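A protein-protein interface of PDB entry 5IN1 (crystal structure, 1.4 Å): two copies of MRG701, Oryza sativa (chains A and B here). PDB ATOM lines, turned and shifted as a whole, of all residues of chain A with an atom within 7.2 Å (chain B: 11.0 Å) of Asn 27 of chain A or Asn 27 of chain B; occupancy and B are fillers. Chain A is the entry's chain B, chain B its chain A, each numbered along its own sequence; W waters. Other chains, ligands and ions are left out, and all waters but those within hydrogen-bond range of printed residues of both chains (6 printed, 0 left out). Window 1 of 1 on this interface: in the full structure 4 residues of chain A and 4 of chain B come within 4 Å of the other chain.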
ATOM      1  N   SER A   2      10.900  -1.779 -14.180  1.00  0.00           N
ATOM      2  CA  SER A   2       9.922  -0.693 -14.243  1.00  0.00           C
ATOM      3  C   SER A   2      10.630   0.645 -14.367  1.00  0.00           C
ATOM      4  O   SER A   2      11.790   0.782 -13.969  1.00  0.00           O
ATOM      5  CB  SER A   2       9.025  -0.686 -13.008  1.00  0.00           C
ATOM      6  OG  SER A   2       9.781  -0.460 -11.825  1.00  0.00           O
ATOM      7  N   SER A  25       5.415   7.266 -11.230  1.00  0.00           N
ATOM      8  CA  SER A  25       5.231   5.832 -11.440  1.00  0.00           C
ATOM      9  C   SER A  25       4.370   5.279 -10.317  1.00  0.00           C
ATOM     10  O   SER A  25       4.617   5.568  -9.139  1.00  0.00           O
ATOM     11  CB  SER A  25       6.566   5.087 -11.469  1.00  0.00           C
ATOM     12  OG  SER A  25       7.442   5.641 -12.442  1.00  0.00           O
ATOM     13  N   GLU A  26       3.382   4.464 -10.667  1.00  0.00           N
ATOM     14  CA  GLU A  26       2.503   3.863  -9.662  1.00  0.00           C
ATOM     15  C   GLU A  26       2.149   2.438 -10.038  1.00  0.00           C
ATOM     16  O   GLU A  26       2.032   2.114 -11.222  1.00  0.00           O
ATOM     17  CB  GLU A  26       1.219   4.672  -9.493  1.00  0.00           C
ATOM     18  CG  GLU A  26       1.396   6.082  -8.943  1.00  0.00           C
ATOM     19  CD  GLU A  26       0.081   6.833  -8.884  1.00  0.00           C
ATOM     20  OE1 GLU A  26      -0.961   6.238  -9.224  1.00  0.00           O
ATOM     21  OE2 GLU A  26       0.087   8.019  -8.509  1.00  0.00           O
ATOM     22  N   ASN A  27       1.972   1.586  -9.031  1.00  0.00           N
ATOM     23  CA  ASN A  27       1.531   0.219  -9.278  1.00  0.00           C
ATOM     24  C   ASN A  27       0.346  -0.116  -8.394  1.00  0.00           C
ATOM     25  O   ASN A  27       0.417   0.042  -7.180  1.00  0.00           O
ATOM     26  CB  ASN A  27       2.687  -0.765  -9.057  1.00  0.00           C
ATOM     27  CG  ASN A  27       2.344  -2.194  -9.466  1.00  0.00           C
ATOM     28  OD1 ASN A  27       1.359  -2.773  -9.006  1.00  0.00           O
ATOM     29  ND2 ASN A  27       3.154  -2.762 -10.363  1.00  0.00           N
ATOM     30  N   LYS A  28      -0.750  -0.531  -9.018  1.00  0.00           N
ATOM     31  CA  LYS A  28      -1.868  -1.168  -8.323  1.00  0.00           C
ATOM     32  C   LYS A  28      -2.294  -2.374  -9.139  1.00  0.00           C
ATOM     33  O   LYS A  28      -2.143  -2.386 -10.371  1.00  0.00           O
ATOM     34  CB  LYS A  28      -3.049  -0.213  -8.128  1.00  0.00           C
ATOM     35  CG  LYS A  28      -2.780   0.956  -7.196  1.00  0.00           C
ATOM     36  CD  LYS A  28      -4.051   1.743  -6.882  1.00  0.00           C
ATOM     37  CE  LYS A  28      -3.798   2.765  -5.773  1.00  0.00           C
ATOM     38  NZ  LYS A  28      -5.021   3.552  -5.426  1.00  0.00           N
ATOM     39  N   GLU A  29      -2.817  -3.388  -8.453  1.00  0.00           N
ATOM     40  CA  GLU A  29      -3.320  -4.600  -9.106  1.00  0.00           C
ATOM     41  C   GLU A  29      -2.299  -5.247 -10.049  1.00  0.00           C
ATOM     42  O   GLU A  29      -2.656  -5.707 -11.139  1.00  0.00           O
ATOM     43  CB  GLU A  29      -4.607  -4.284  -9.869  1.00  0.00           C
ATOM     44  CG  GLU A  29      -5.752  -3.846  -8.978  1.00  0.00           C
ATOM     45  CD  GLU A  29      -6.007  -4.813  -7.830  1.00  0.00           C
ATOM     46  OE1 GLU A  29      -5.895  -6.041  -8.035  1.00  0.00           O
ATOM     47  OE2 GLU A  29      -6.325  -4.343  -6.715  1.00  0.00           O
ATOM     48  N   ASP A  30      -1.043  -5.283  -9.609  1.00  0.00           N
ATOM     49  CA  ASP A  30       0.058  -5.886 -10.351  1.00  0.00           C
ATOM     50  C   ASP A  30       0.166  -5.271 -11.743  1.00  0.00           C
ATOM     51  O   ASP A  30       0.373  -5.978 -12.730  1.00  0.00           O
ATOM     52  CB  ASP A  30      -0.119  -7.409 -10.443  1.00  0.00           C
ATOM     53  CG  ASP A  30       1.198  -8.148 -10.684  1.00  0.00           C
ATOM     54  OD1 ASP A  30       2.281  -7.581 -10.429  1.00  0.00           O
ATOM     55  OD2 ASP A  30       1.149  -9.316 -11.128  1.00  0.00           O
ATOM     56  N   GLU A  31       0.004  -3.953 -11.813  1.00  0.00           N
ATOM     57  CA  GLU A  31       0.151  -3.218 -13.069  1.00  0.00           C
ATOM     58  C   GLU A  31       0.747  -1.830 -12.836  1.00  0.00           C
ATOM     59  O   GLU A  31       0.281  -1.057 -11.991  1.00  0.00           O
ATOM     60  CB  GLU A  31      -1.193  -3.100 -13.779  1.00  0.00           C
ATOM     61  CG  GLU A  31      -1.173  -2.281 -15.068  1.00  0.00           C
ATOM     62  CD  GLU A  31      -2.442  -2.457 -15.867  1.00  0.00           C
ATOM     63  OE1 GLU A  31      -2.832  -3.626 -16.082  1.00  0.00           O
ATOM     64  OE2 GLU A  31      -3.070  -1.445 -16.254  1.00  0.00           O
ATOM     65  N   TRP A  32       1.771  -1.518 -13.615  1.00  0.00           N
ATOM     66  CA  TRP A  32       2.385  -0.203 -13.573  1.00  0.00           C
ATOM     67  C   TRP A  32       1.664   0.797 -14.455  1.00  0.00           C
ATOM     68  O   TRP A  32       1.202   0.478 -15.557  1.00  0.00           O
ATOM     69  CB  TRP A  32       3.845  -0.287 -13.992  1.00  0.00           C
ATOM     70  CG  TRP A  32       4.712  -0.889 -12.963  1.00  0.00           C
ATOM     71  CD1 TRP A  32       5.160  -2.179 -12.918  1.00  0.00           C
ATOM     72  CD2 TRP A  32       5.237  -0.237 -11.802  1.00  0.00           C
ATOM     73  NE1 TRP A  32       5.945  -2.362 -11.803  1.00  0.00           N
ATOM     74  CE2 TRP A  32       6.003  -1.188 -11.097  1.00  0.00           C
ATOM     75  CE3 TRP A  32       5.132   1.062 -11.290  1.00  0.00           C
ATOM     76  CZ2 TRP A  32       6.671  -0.878  -9.909  1.00  0.00           C
ATOM     77  CZ3 TRP A  32       5.789   1.371 -10.110  1.00  0.00           C
ATOM     78  CH2 TRP A  32       6.549   0.402  -9.430  1.00  0.00           C
ATOM     79  N   ARG A  33       1.566   2.026 -13.978  1.00  0.00           N
ATOM     80  CA  ARG A  33       1.205   3.126 -14.862  1.00  0.00           C
ATOM     81  C   ARG A  33       2.179   4.262 -14.632  1.00  0.00           C
ATOM     82  O   ARG A  33       2.733   4.445 -13.544  1.00  0.00           O
ATOM     83  CB  ARG A  33      -0.239   3.588 -14.654  1.00  0.00           C
ATOM     84  CG  ARG A  33      -0.535   4.207 -13.291  1.00  0.00           C
ATOM     85  CD  ARG A  33      -1.949   4.769 -13.256  1.00  0.00           C
ATOM     86  NE  ARG A  33      -2.184   5.556 -12.051  1.00  0.00           N
ATOM     87  CZ  ARG A  33      -3.156   6.449 -11.904  1.00  0.00           C
ATOM     88  NH1 ARG A  33      -3.996   6.697 -12.903  1.00  0.00           N
ATOM     89  NH2 ARG A  33      -3.278   7.104 -10.750  1.00  0.00           N
ATOM     90  N   TYR A  34       2.393   5.024 -15.689  1.00  0.00           N
ATOM     91  CA  TYR A  34       3.382   6.086 -15.717  1.00  0.00           C
ATOM     92  C   TYR A  34       2.753   7.371 -16.236  1.00  0.00           C
ATOM     93  O   TYR A  34       2.103   7.377 -17.286  1.00  0.00           O
ATOM     94  CB  TYR A  34       4.555   5.681 -16.598  1.00  0.00           C
ATOM     95  CG  TYR A  34       5.176   4.360 -16.197  1.00  0.00           C
ATOM     96  CD1 TYR A  34       6.078   4.299 -15.140  1.00  0.00           C
ATOM     97  CD2 TYR A  34       4.870   3.179 -16.862  1.00  0.00           C
ATOM     98  CE1 TYR A  34       6.648   3.104 -14.758  1.00  0.00           C
ATOM     99  CE2 TYR A  34       5.440   1.973 -16.489  1.00  0.00           C
ATOM    100  CZ  TYR A  34       6.333   1.950 -15.446  1.00  0.00           C
ATOM    101  OH  TYR A  34       6.912   0.765 -15.073  1.00  0.00           O
ATOM    102  N   SER B   2       9.307  -7.729  -4.810  1.00  0.00           N
ATOM    103  CA  SER B   2       8.129  -7.269  -4.080  1.00  0.00           C
ATOM    104  C   SER B   2       7.154  -8.422  -3.846  1.00  0.00           C
ATOM    105  O   SER B   2       7.027  -9.320  -4.676  1.00  0.00           O
ATOM    106  CB  SER B   2       7.430  -6.142  -4.837  1.00  0.00           C
ATOM    107  OG  SER B   2       7.001  -6.581  -6.113  1.00  0.00           O
ATOM    108  N   PHE B   3       6.453  -8.387  -2.721  1.00  0.00           N
ATOM    109  CA  PHE B   3       5.543  -9.473  -2.373  1.00  0.00           C
ATOM    110  C   PHE B   3       4.277  -9.380  -3.216  1.00  0.00           C
ATOM    111  O   PHE B   3       3.869  -8.287  -3.636  1.00  0.00           O
ATOM    112  CB  PHE B   3       5.187  -9.442  -0.879  1.00  0.00           C
ATOM    113  CG  PHE B   3       6.374  -9.529   0.036  1.00  0.00           C
ATOM    114  CD1 PHE B   3       7.047 -10.724   0.225  1.00  0.00           C
ATOM    115  CD2 PHE B   3       6.802  -8.415   0.738  1.00  0.00           C
ATOM    116  CE1 PHE B   3       8.126 -10.795   1.083  1.00  0.00           C
ATOM    117  CE2 PHE B   3       7.890  -8.487   1.591  1.00  0.00           C
ATOM    118  CZ  PHE B   3       8.552  -9.670   1.761  1.00  0.00           C
ATOM    119  N   LYS B   4       3.656 -10.523  -3.452  1.00  0.00           N
ATOM    120  CA  LYS B   4       2.501 -10.603  -4.337  1.00  0.00           C
ATOM    121  C   LYS B   4       1.230 -10.911  -3.566  1.00  0.00           C
ATOM    122  O   LYS B   4       1.267 -11.506  -2.478  1.00  0.00           O
ATOM    123  CB  LYS B   4       2.718 -11.675  -5.410  1.00  0.00           C
ATOM    124  CG  LYS B   4       3.930 -11.433  -6.283  1.00  0.00           C
ATOM    125  CD  LYS B   4       3.732 -10.196  -7.159  1.00  0.00           C
ATOM    126  CE  LYS B   4       4.862  -9.999  -8.171  1.00  0.00           C
ATOM    127  NZ  LYS B   4       6.042  -9.294  -7.580  1.00  0.00           N
ATOM    128  N   GLU B   5       0.098 -10.520  -4.134  1.00  0.00           N
ATOM    129  CA  GLU B   5      -1.194 -10.849  -3.575  1.00  0.00           C
ATOM    130  C   GLU B   5      -1.287 -12.354  -3.353  1.00  0.00           C
ATOM    131  O   GLU B   5      -0.953 -13.140  -4.236  1.00  0.00           O
ATOM    132  CB  GLU B   5      -2.313 -10.382  -4.503  1.00  0.00           C
ATOM    133  CG  GLU B   5      -3.677 -10.567  -3.925  1.00  0.00           C
ATOM    134  CD  GLU B   5      -4.765 -10.223  -4.910  1.00  0.00           C
ATOM    135  OE1 GLU B   5      -4.523  -9.346  -5.767  1.00  0.00           O
ATOM    136  OE2 GLU B   5      -5.840 -10.860  -4.847  1.00  0.00           O
ATOM    137  N   VAL B  22      -0.474 -11.551   2.228  1.00  0.00           N
ATOM    138  CA  VAL B  22      -0.632 -10.295   1.508  1.00  0.00           C
ATOM    139  C   VAL B  22      -1.978 -10.277   0.785  1.00  0.00           C
ATOM    140  O   VAL B  22      -2.246 -11.143  -0.044  1.00  0.00           O
ATOM    141  CB  VAL B  22       0.510 -10.094   0.501  1.00  0.00           C
ATOM    142  CG1 VAL B  22       0.282  -8.811  -0.307  1.00  0.00           C
ATOM    143  CG2 VAL B  22       1.838 -10.062   1.215  1.00  0.00           C
ATOM    144  N   LYS B  24      -3.223  -7.215  -0.639  1.00  0.00           N
ATOM    145  CA  LYS B  24      -3.063  -6.244  -1.723  1.00  0.00           C
ATOM    146  C   LYS B  24      -1.653  -5.672  -1.685  1.00  0.00           C
ATOM    147  O   LYS B  24      -1.096  -5.487  -0.608  1.00  0.00           O
ATOM    148  CB  LYS B  24      -4.109  -5.125  -1.596  1.00  0.00           C
ATOM    149  CG  LYS B  24      -5.504  -5.537  -2.081  1.00  0.00           C
ATOM    150  CD  LYS B  24      -6.575  -4.471  -1.848  1.00  0.00           C
ATOM    151  CE  LYS B  24      -7.947  -5.118  -1.623  1.00  0.00           C
ATOM    152  NZ  LYS B  24      -8.921  -4.872  -2.729  1.00  0.00           N
ATOM    153  N   SER B  25      -1.085  -5.393  -2.858  1.00  0.00           N
ATOM    154  CA  SER B  25       0.217  -4.743  -2.981  1.00  0.00           C
ATOM    155  C   SER B  25       0.051  -3.476  -3.813  1.00  0.00           C
ATOM    156  O   SER B  25      -0.623  -3.491  -4.847  1.00  0.00           O
ATOM    157  CB  SER B  25       1.249  -5.663  -3.645  1.00  0.00           C
ATOM    158  OG  SER B  25       1.321  -6.932  -3.000  1.00  0.00           O
ATOM    159  N   GLU B  26       0.647  -2.377  -3.363  1.00  0.00           N
ATOM    160  CA  GLU B  26       0.601  -1.120  -4.116  1.00  0.00           C
ATOM    161  C   GLU B  26       1.941  -0.430  -4.065  1.00  0.00           C
ATOM    162  O   GLU B  26       2.663  -0.551  -3.077  1.00  0.00           O
ATOM    163  CB  GLU B  26      -0.468  -0.174  -3.563  1.00  0.00           C
ATOM    164  CG  GLU B  26      -1.900  -0.663  -3.711  1.00  0.00           C
ATOM    165  CD  GLU B  26      -2.890   0.258  -3.022  1.00  0.00           C
ATOM    166  OE1 GLU B  26      -2.445   1.252  -2.409  1.00  0.00           O
ATOM    167  OE2 GLU B  26      -4.106  -0.014  -3.086  1.00  0.00           O
ATOM    168  N   ASN B  27       2.276   0.310  -5.123  1.00  0.00           N
ATOM    169  CA  ASN B  27       3.491   1.114  -5.120  1.00  0.00           C
ATOM    170  C   ASN B  27       3.186   2.541  -5.528  1.00  0.00           C
ATOM    171  O   ASN B  27       2.558   2.773  -6.561  1.00  0.00           O
ATOM    172  CB  ASN B  27       4.550   0.491  -6.041  1.00  0.00           C
ATOM    173  CG  ASN B  27       5.904   1.160  -5.919  1.00  0.00           C
ATOM    174  OD1 ASN B  27       6.033   2.379  -6.071  1.00  0.00           O
ATOM    175  ND2 ASN B  27       6.928   0.369  -5.632  1.00  0.00           N
ATOM    176  N   LYS B  28       3.616   3.483  -4.691  1.00  0.00           N
ATOM    177  CA  LYS B  28       3.647   4.907  -5.014  1.00  0.00           C
ATOM    178  C   LYS B  28       4.927   5.470  -4.452  1.00  0.00           C
ATOM    179  O   LYS B  28       5.436   4.976  -3.442  1.00  0.00           O
ATOM    180  CB  LYS B  28       2.454   5.662  -4.427  1.00  0.00           C
ATOM    181  CG  LYS B  28       1.140   5.429  -5.109  1.00  0.00           C
ATOM    182  CD  LYS B  28       0.115   6.460  -4.655  1.00  0.00           C
ATOM    183  CE  LYS B  28      -1.233   6.203  -5.299  1.00  0.00           C
ATOM    184  NZ  LYS B  28      -2.231   7.223  -4.874  1.00  0.00           N
ATOM    185  N   GLU B  29       5.438   6.511  -5.103  1.00  0.00           N
ATOM    186  CA  GLU B  29       6.650   7.195  -4.666  1.00  0.00           C
ATOM    187  C   GLU B  29       7.794   6.229  -4.398  1.00  0.00           C
ATOM    188  O   GLU B  29       8.501   6.367  -3.400  1.00  0.00           O
ATOM    189  CB  GLU B  29       6.365   8.037  -3.418  1.00  0.00           C
ATOM    190  CG  GLU B  29       5.293   9.099  -3.624  1.00  0.00           C
ATOM    191  CD  GLU B  29       5.660  10.113  -4.700  1.00  0.00           C
ATOM    192  OE1 GLU B  29       6.859  10.257  -5.018  1.00  0.00           O
ATOM    193  OE2 GLU B  29       4.742  10.768  -5.238  1.00  0.00           O
ATOM    194  N   ASP B  30       7.950   5.247  -5.283  1.00  0.00           N
ATOM    195  CA  ASP B  30       9.071   4.316  -5.233  1.00  0.00           C
ATOM    196  C   ASP B  30       9.089   3.524  -3.918  1.00  0.00           C
ATOM    197  O   ASP B  30      10.142   3.312  -3.318  1.00  0.00           O
ATOM    198  CB  ASP B  30      10.379   5.089  -5.423  1.00  0.00           C
ATOM    199  CG  ASP B  30      11.537   4.204  -5.790  1.00  0.00           C
ATOM    200  OD1 ASP B  30      11.324   3.118  -6.366  1.00  0.00           O
ATOM    201  OD2 ASP B  30      12.679   4.610  -5.492  1.00  0.00           O
ATOM    202  N   GLU B  31       7.910   3.086  -3.490  1.00  0.00           N
ATOM    203  CA  GLU B  31       7.746   2.390  -2.220  1.00  0.00           C
ATOM    204  C   GLU B  31       6.577   1.423  -2.307  1.00  0.00           C
ATOM    205  O   GLU B  31       5.457   1.816  -2.608  1.00  0.00           O
ATOM    206  CB  GLU B  31       7.519   3.404  -1.088  1.00  0.00           C
ATOM    207  CG  GLU B  31       7.423   2.833   0.324  1.00  0.00           C
ATOM    208  CD  GLU B  31       7.600   3.911   1.394  1.00  0.00           C
ATOM    209  OE1 GLU B  31       8.651   4.598   1.383  1.00  0.00           O
ATOM    210  OE2 GLU B  31       6.684   4.082   2.222  1.00  0.00           O
ATOM    211  N   TRP B  32       6.842   0.154  -2.030  1.00  0.00           N
ATOM    212  CA  TRP B  32       5.774  -0.830  -1.933  1.00  0.00           C
ATOM    213  C   TRP B  32       5.087  -0.773  -0.565  1.00  0.00           C
ATOM    214  O   TRP B  32       5.751  -0.653   0.471  1.00  0.00           O
ATOM    215  CB  TRP B  32       6.320  -2.241  -2.178  1.00  0.00           C
ATOM    216  CG  TRP B  32       6.566  -2.543  -3.632  1.00  0.00           C
ATOM    217  CD1 TRP B  32       7.772  -2.545  -4.283  1.00  0.00           C
ATOM    218  CD2 TRP B  32       5.578  -2.871  -4.614  1.00  0.00           C
ATOM    219  NE1 TRP B  32       7.588  -2.854  -5.608  1.00  0.00           N
ATOM    220  CE2 TRP B  32       6.255  -3.056  -5.845  1.00  0.00           C
ATOM    221  CE3 TRP B  32       4.192  -3.016  -4.579  1.00  0.00           C
ATOM    222  CZ2 TRP B  32       5.589  -3.391  -7.027  1.00  0.00           C
ATOM    223  CZ3 TRP B  32       3.526  -3.354  -5.746  1.00  0.00           C
ATOM    224  CH2 TRP B  32       4.231  -3.528  -6.965  1.00  0.00           C
ATOM    225  N   ARG B  33       3.760  -0.862  -0.556  1.00  0.00           N
ATOM    226  CA  ARG B  33       3.042  -1.138   0.692  1.00  0.00           C
ATOM    227  C   ARG B  33       2.146  -2.341   0.488  1.00  0.00           C
ATOM    228  O   ARG B  33       1.722  -2.639  -0.636  1.00  0.00           O
ATOM    229  CB  ARG B  33       2.229   0.073   1.175  1.00  0.00           C
ATOM    230  CG  ARG B  33       1.083   0.497   0.268  1.00  0.00           C
ATOM    231  CD  ARG B  33       0.285   1.618   0.919  1.00  0.00           C
ATOM    232  NE  ARG B  33      -0.988   1.868   0.238  1.00  0.00           N
ATOM    233  CZ  ARG B  33      -2.000   2.539   0.775  1.00  0.00           C
ATOM    234  NH1 ARG B  33      -1.895   3.026   2.007  1.00  0.00           N
ATOM    235  NH2 ARG B  33      -3.119   2.727   0.076  1.00  0.00           N
ATOM    236  N   TYR B  34       1.874  -3.046   1.579  1.00  0.00           N
ATOM    237  CA  TYR B  34       1.201  -4.328   1.542  1.00  0.00           C
ATOM    238  C   TYR B  34       0.108  -4.348   2.591  1.00  0.00           C
ATOM    239  O   TYR B  34       0.376  -4.070   3.764  1.00  0.00           O
ATOM    240  CB  TYR B  34       2.194  -5.457   1.806  1.00  0.00           C
ATOM    241  CG  TYR B  34       3.391  -5.449   0.884  1.00  0.00           C
ATOM    242  CD1 TYR B  34       3.297  -5.962  -0.400  1.00  0.00           C
ATOM    243  CD2 TYR B  34       4.604  -4.917   1.284  1.00  0.00           C
ATOM    244  CE1 TYR B  34       4.393  -5.950  -1.257  1.00  0.00           C
ATOM    245  CE2 TYR B  34       5.694  -4.911   0.444  1.00  0.00           C
ATOM    246  CZ  TYR B  34       5.586  -5.439  -0.820  1.00  0.00           C
ATOM    247  OH  TYR B  34       6.678  -5.422  -1.668  1.00  0.00           O
ATOM    248  N   HIS B  35      -1.108  -4.689   2.184  1.00  0.00           N
ATOM    249  CA  HIS B  35      -2.196  -4.818   3.139  1.00  0.00           C
ATOM    250  C   HIS B  35      -2.197  -6.276   3.530  1.00  0.00           C
ATOM    251  O   HIS B  35      -2.395  -7.142   2.682  1.00  0.00           O
ATOM    252  CB  HIS B  35      -3.552  -4.388   2.551  1.00  0.00           C
ATOM    253  CG  HIS B  35      -4.553  -3.973   3.583  1.00  0.00           C
ATOM    254  ND1 HIS B  35      -5.453  -4.852   4.155  1.00  0.00           N
ATOM    255  CD2 HIS B  35      -4.800  -2.765   4.155  1.00  0.00           C
ATOM    256  CE1 HIS B  35      -6.209  -4.204   5.024  1.00  0.00           C
ATOM    257  NE2 HIS B  35      -5.836  -2.939   5.042  1.00  0.00           N
ATOM    258  N   TRP B  48      -2.010  -1.846   6.407  1.00  0.00           N
ATOM    259  CA  TRP B  48      -0.939  -1.559   5.472  1.00  0.00           C
ATOM    260  C   TRP B  48       0.394  -1.544   6.183  1.00  0.00           C
ATOM    261  O   TRP B  48       0.546  -0.885   7.217  1.00  0.00           O
ATOM    262  CB  TRP B  48      -1.117  -0.190   4.807  1.00  0.00           C
ATOM    263  CG  TRP B  48      -2.237  -0.072   3.844  1.00  0.00           C
ATOM    264  CD1 TRP B  48      -3.408   0.610   4.031  1.00  0.00           C
ATOM    265  CD2 TRP B  48      -2.297  -0.615   2.523  1.00  0.00           C
ATOM    266  NE1 TRP B  48      -4.192   0.509   2.916  1.00  0.00           N
ATOM    267  CE2 TRP B  48      -3.535  -0.238   1.973  1.00  0.00           C
ATOM    268  CE3 TRP B  48      -1.418  -1.387   1.751  1.00  0.00           C
ATOM    269  CZ2 TRP B  48      -3.924  -0.612   0.683  1.00  0.00           C
ATOM    270  CZ3 TRP B  48      -1.803  -1.760   0.470  1.00  0.00           C
ATOM    271  CH2 TRP B  48      -3.047  -1.369  -0.051  1.00  0.00           C
ATOM    272  N   VAL B  49       1.367  -2.258   5.631  1.00  0.00           N
ATOM    273  CA  VAL B  49       2.725  -2.189   6.139  1.00  0.00           C
ATOM    274  C   VAL B  49       3.733  -2.019   5.017  1.00  0.00           C
ATOM    275  O   VAL B  49       3.477  -2.378   3.857  1.00  0.00           O
ATOM    276  CB  VAL B  49       3.085  -3.458   6.946  1.00  0.00           C
ATOM    277  CG1 VAL B  49       2.114  -3.658   8.120  1.00  0.00           C
ATOM    278  CG2 VAL B  49       3.094  -4.668   6.040  1.00  0.00           C
ATOM    279  N   THR B  50       4.905  -1.511   5.366  1.00  0.00           N
ATOM    280  CA  THR B  50       5.978  -1.416   4.398  1.00  0.00           C
ATOM    281  C   THR B  50       6.984  -2.552   4.585  1.00  0.00           C
ATOM    282  O   THR B  50       6.832  -3.404   5.479  1.00  0.00           O
ATOM    283  CB  THR B  50       6.652  -0.036   4.475  1.00  0.00           C
ATOM    284  OG1 THR B  50       6.796   0.335   5.845  1.00  0.00           O
ATOM    285  CG2 THR B  50       5.752   0.988   3.788  1.00  0.00           C
ATOM    286  N   ASN B  51       7.981  -2.596   3.709  1.00  0.00           N
ATOM    287  CA  ASN B  51       8.879  -3.731   3.604  1.00  0.00           C
ATOM    288  C   ASN B  51       9.610  -4.080   4.897  1.00  0.00           C
ATOM    289  O   ASN B  51       9.888  -5.254   5.186  1.00  0.00           O
ATOM    290  CB  ASN B  51       9.887  -3.450   2.487  1.00  0.00           C
ATOM    291  CG  ASN B  51      10.836  -4.581   2.267  1.00  0.00           C
ATOM    292  OD1 ASN B  51      10.442  -5.631   1.778  1.00  0.00           O
ATOM    293  ND2 ASN B  51      12.108  -4.375   2.608  1.00  0.00           N
HETATM  294  O   HOH W   1       6.699   4.367  -7.761  1.00  0.00           O
HETATM  295  O   HOH W   2      -3.220  -3.669  -5.712  1.00  0.00           O
HETATM  296  O   HOH W   3      -5.056  -1.940  -4.620  1.00  0.00           O
HETATM  297  O   HOH W   4      -0.615   2.999  -5.982  1.00  0.00           O
HETATM  298  O   HOH W   5       0.308  -4.482  -7.258  1.00  0.00           O
HETATM  299  O   HOH W   6       4.435   7.731  -7.406  1.00  0.00           O
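Glu 26 of chain A touches Lys 28 of chain B, and with the chains exchanged Lys 28 of chain A touches Glu 26 of chain B. Asn 27 of chain A touches its own counterpart, Asn 27 of chain B. Asn 27 of chain A touches Trp 32 of chain B, and with the chains exchanged Trp 32 of chain A touches Asn 27 of chain B. Trp 32 of chain B touches its own counterpart, Trp 32 of chain A. Positions printed for both chains: 2, 25, 26, 27, 28, 29, 30, 31, 32, 33 and 34. Of the 8 pairs that touch across the chains among the printed residues, 8 have their exchanged pair printed and touching as well.
The side-chain carboxylate of Glu 26 of chain A lies within salt-bridge range of the guanidinium group of Arg 33 of chain A (2.9 Å). The guanidinium group (NH2) of Arg 33 of chain B lies within salt-bridge range of the side-chain carboxylate (OE1) of Glu 26 of chain B (3.0 Å). The backbone NH (N) of Glu 31 of chain A sits at hydrogen-bond distance from the side-chain amide oxygen (OD1) of Asn 27 of chain A, at 3.3 Å. The indole nitrogen (NE1) of Trp 32 of chain B lies close to the side-chain amide nitrogen (ND2) of Asn 27 of chain B, 3.3 Å away. OD1 of Asn 27 of chain B is in hydrogen-bond range of N of Glu 31 of chain B (3.3 Å).
Among the printed residues, pairs that only touch across the chains: Asn 27 of chain A with Glu 26 of chain B (3.3 Å), Glu 26 of chain A with Asn 27 of chain B (3.3 Å), Asn 27 of chain A with Trp 32 of chain B (3.4 Å), Trp 32 of chain A with Asn 27 of chain B (3.6 Å), Lys 28 of chain A with Glu 26 of chain B (3.8 Å), Glu 26 of chain A with Lys 28 of chain B (3.9 Å) and Trp 32 of chain A with Trp 32 of chain B (3.97 Å).
Of the 21 printed residues of chain B, 4 touch a printed residue of chain A. Printed residues of chain B that touch a printed residue of chain A: Glu 26, Asn 27, Lys 28 and Trp 32. Hydrophobic or aromatic side chains of chain B within 4 Å of the printed part of chain A: Trp 32. Along chain B the printed residues that touch a printed residue of chain A span positions 26 to 32. Of the 11 printed residues of chain A, 4 touch a printed residue of chain B. Hydrophobic or aromatic side chains of chain A within 4 Å of the printed part of chain B: Trp 32. Among the printed residues, no Asp or Glu carboxylate lies within 4 Å of a Lys or Arg side-chain nitrogen of the other chain.
Water W3 bridges OE2 of Glu 26 of chain B (2.6 Å) and OE2 of Glu 29 of chain A (3.4 Å). Water W5 lies within hydrogen-bond range of OD1 of Asn 27 of chain A (2.7 Å), O of Ser 25 of chain B (2.8 Å) and N of Asp 30 of chain A (2.8 Å). Water W1 lies within hydrogen-bond range of the side-chain amide oxygen of Asn 27 of chain B (2.7 Å), the backbone carbonyl oxygen of Ser 25 of chain A (2.8 Å) and the backbone NH of Asp 30 of chain B (2.9 Å). Water W6 bridges the backbone carbonyl oxygen of Ser 25 of chain A and the backbone NH of Glu 29 of chain B.
Of chain B, only Asn 27 and Lys 28 come within 4 Å of Glu 26 of chain A. Asn 27 of chain A touches just these residues of chain B: Glu 26 (3.3 Å), Asn 27 (2.8 Å) and Trp 32 (3.4 Å). Lys 28 of chain A touches just one residue of chain B: Glu 26 (3.8 Å). No residue of chain B comes within 4 Å of Asp 30 of chain A. Printed residues of chain A within 4 Å of Glu 26 of chain B: Asn 27 and Lys 28. Asn 27 of chain B touches three residues of chain A. Printed residues of chain A within 4 Å of Trp 32 of chain B: Asn 27 (3.4 Å) and Trp 32 (3.97 Å). Arg 33 of chain B touches none of the printed residues of chain A. The nearest residue of chain B that does not touch Asn 27 of chain A is Ser 25 of chain B (4.4 Å).
The backbone NH (N) of Asn 27 of chain B lies within hydrogen-bond range of the backbone carbonyl oxygen (O) of Asn 27 of chain A (2.8 Å).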
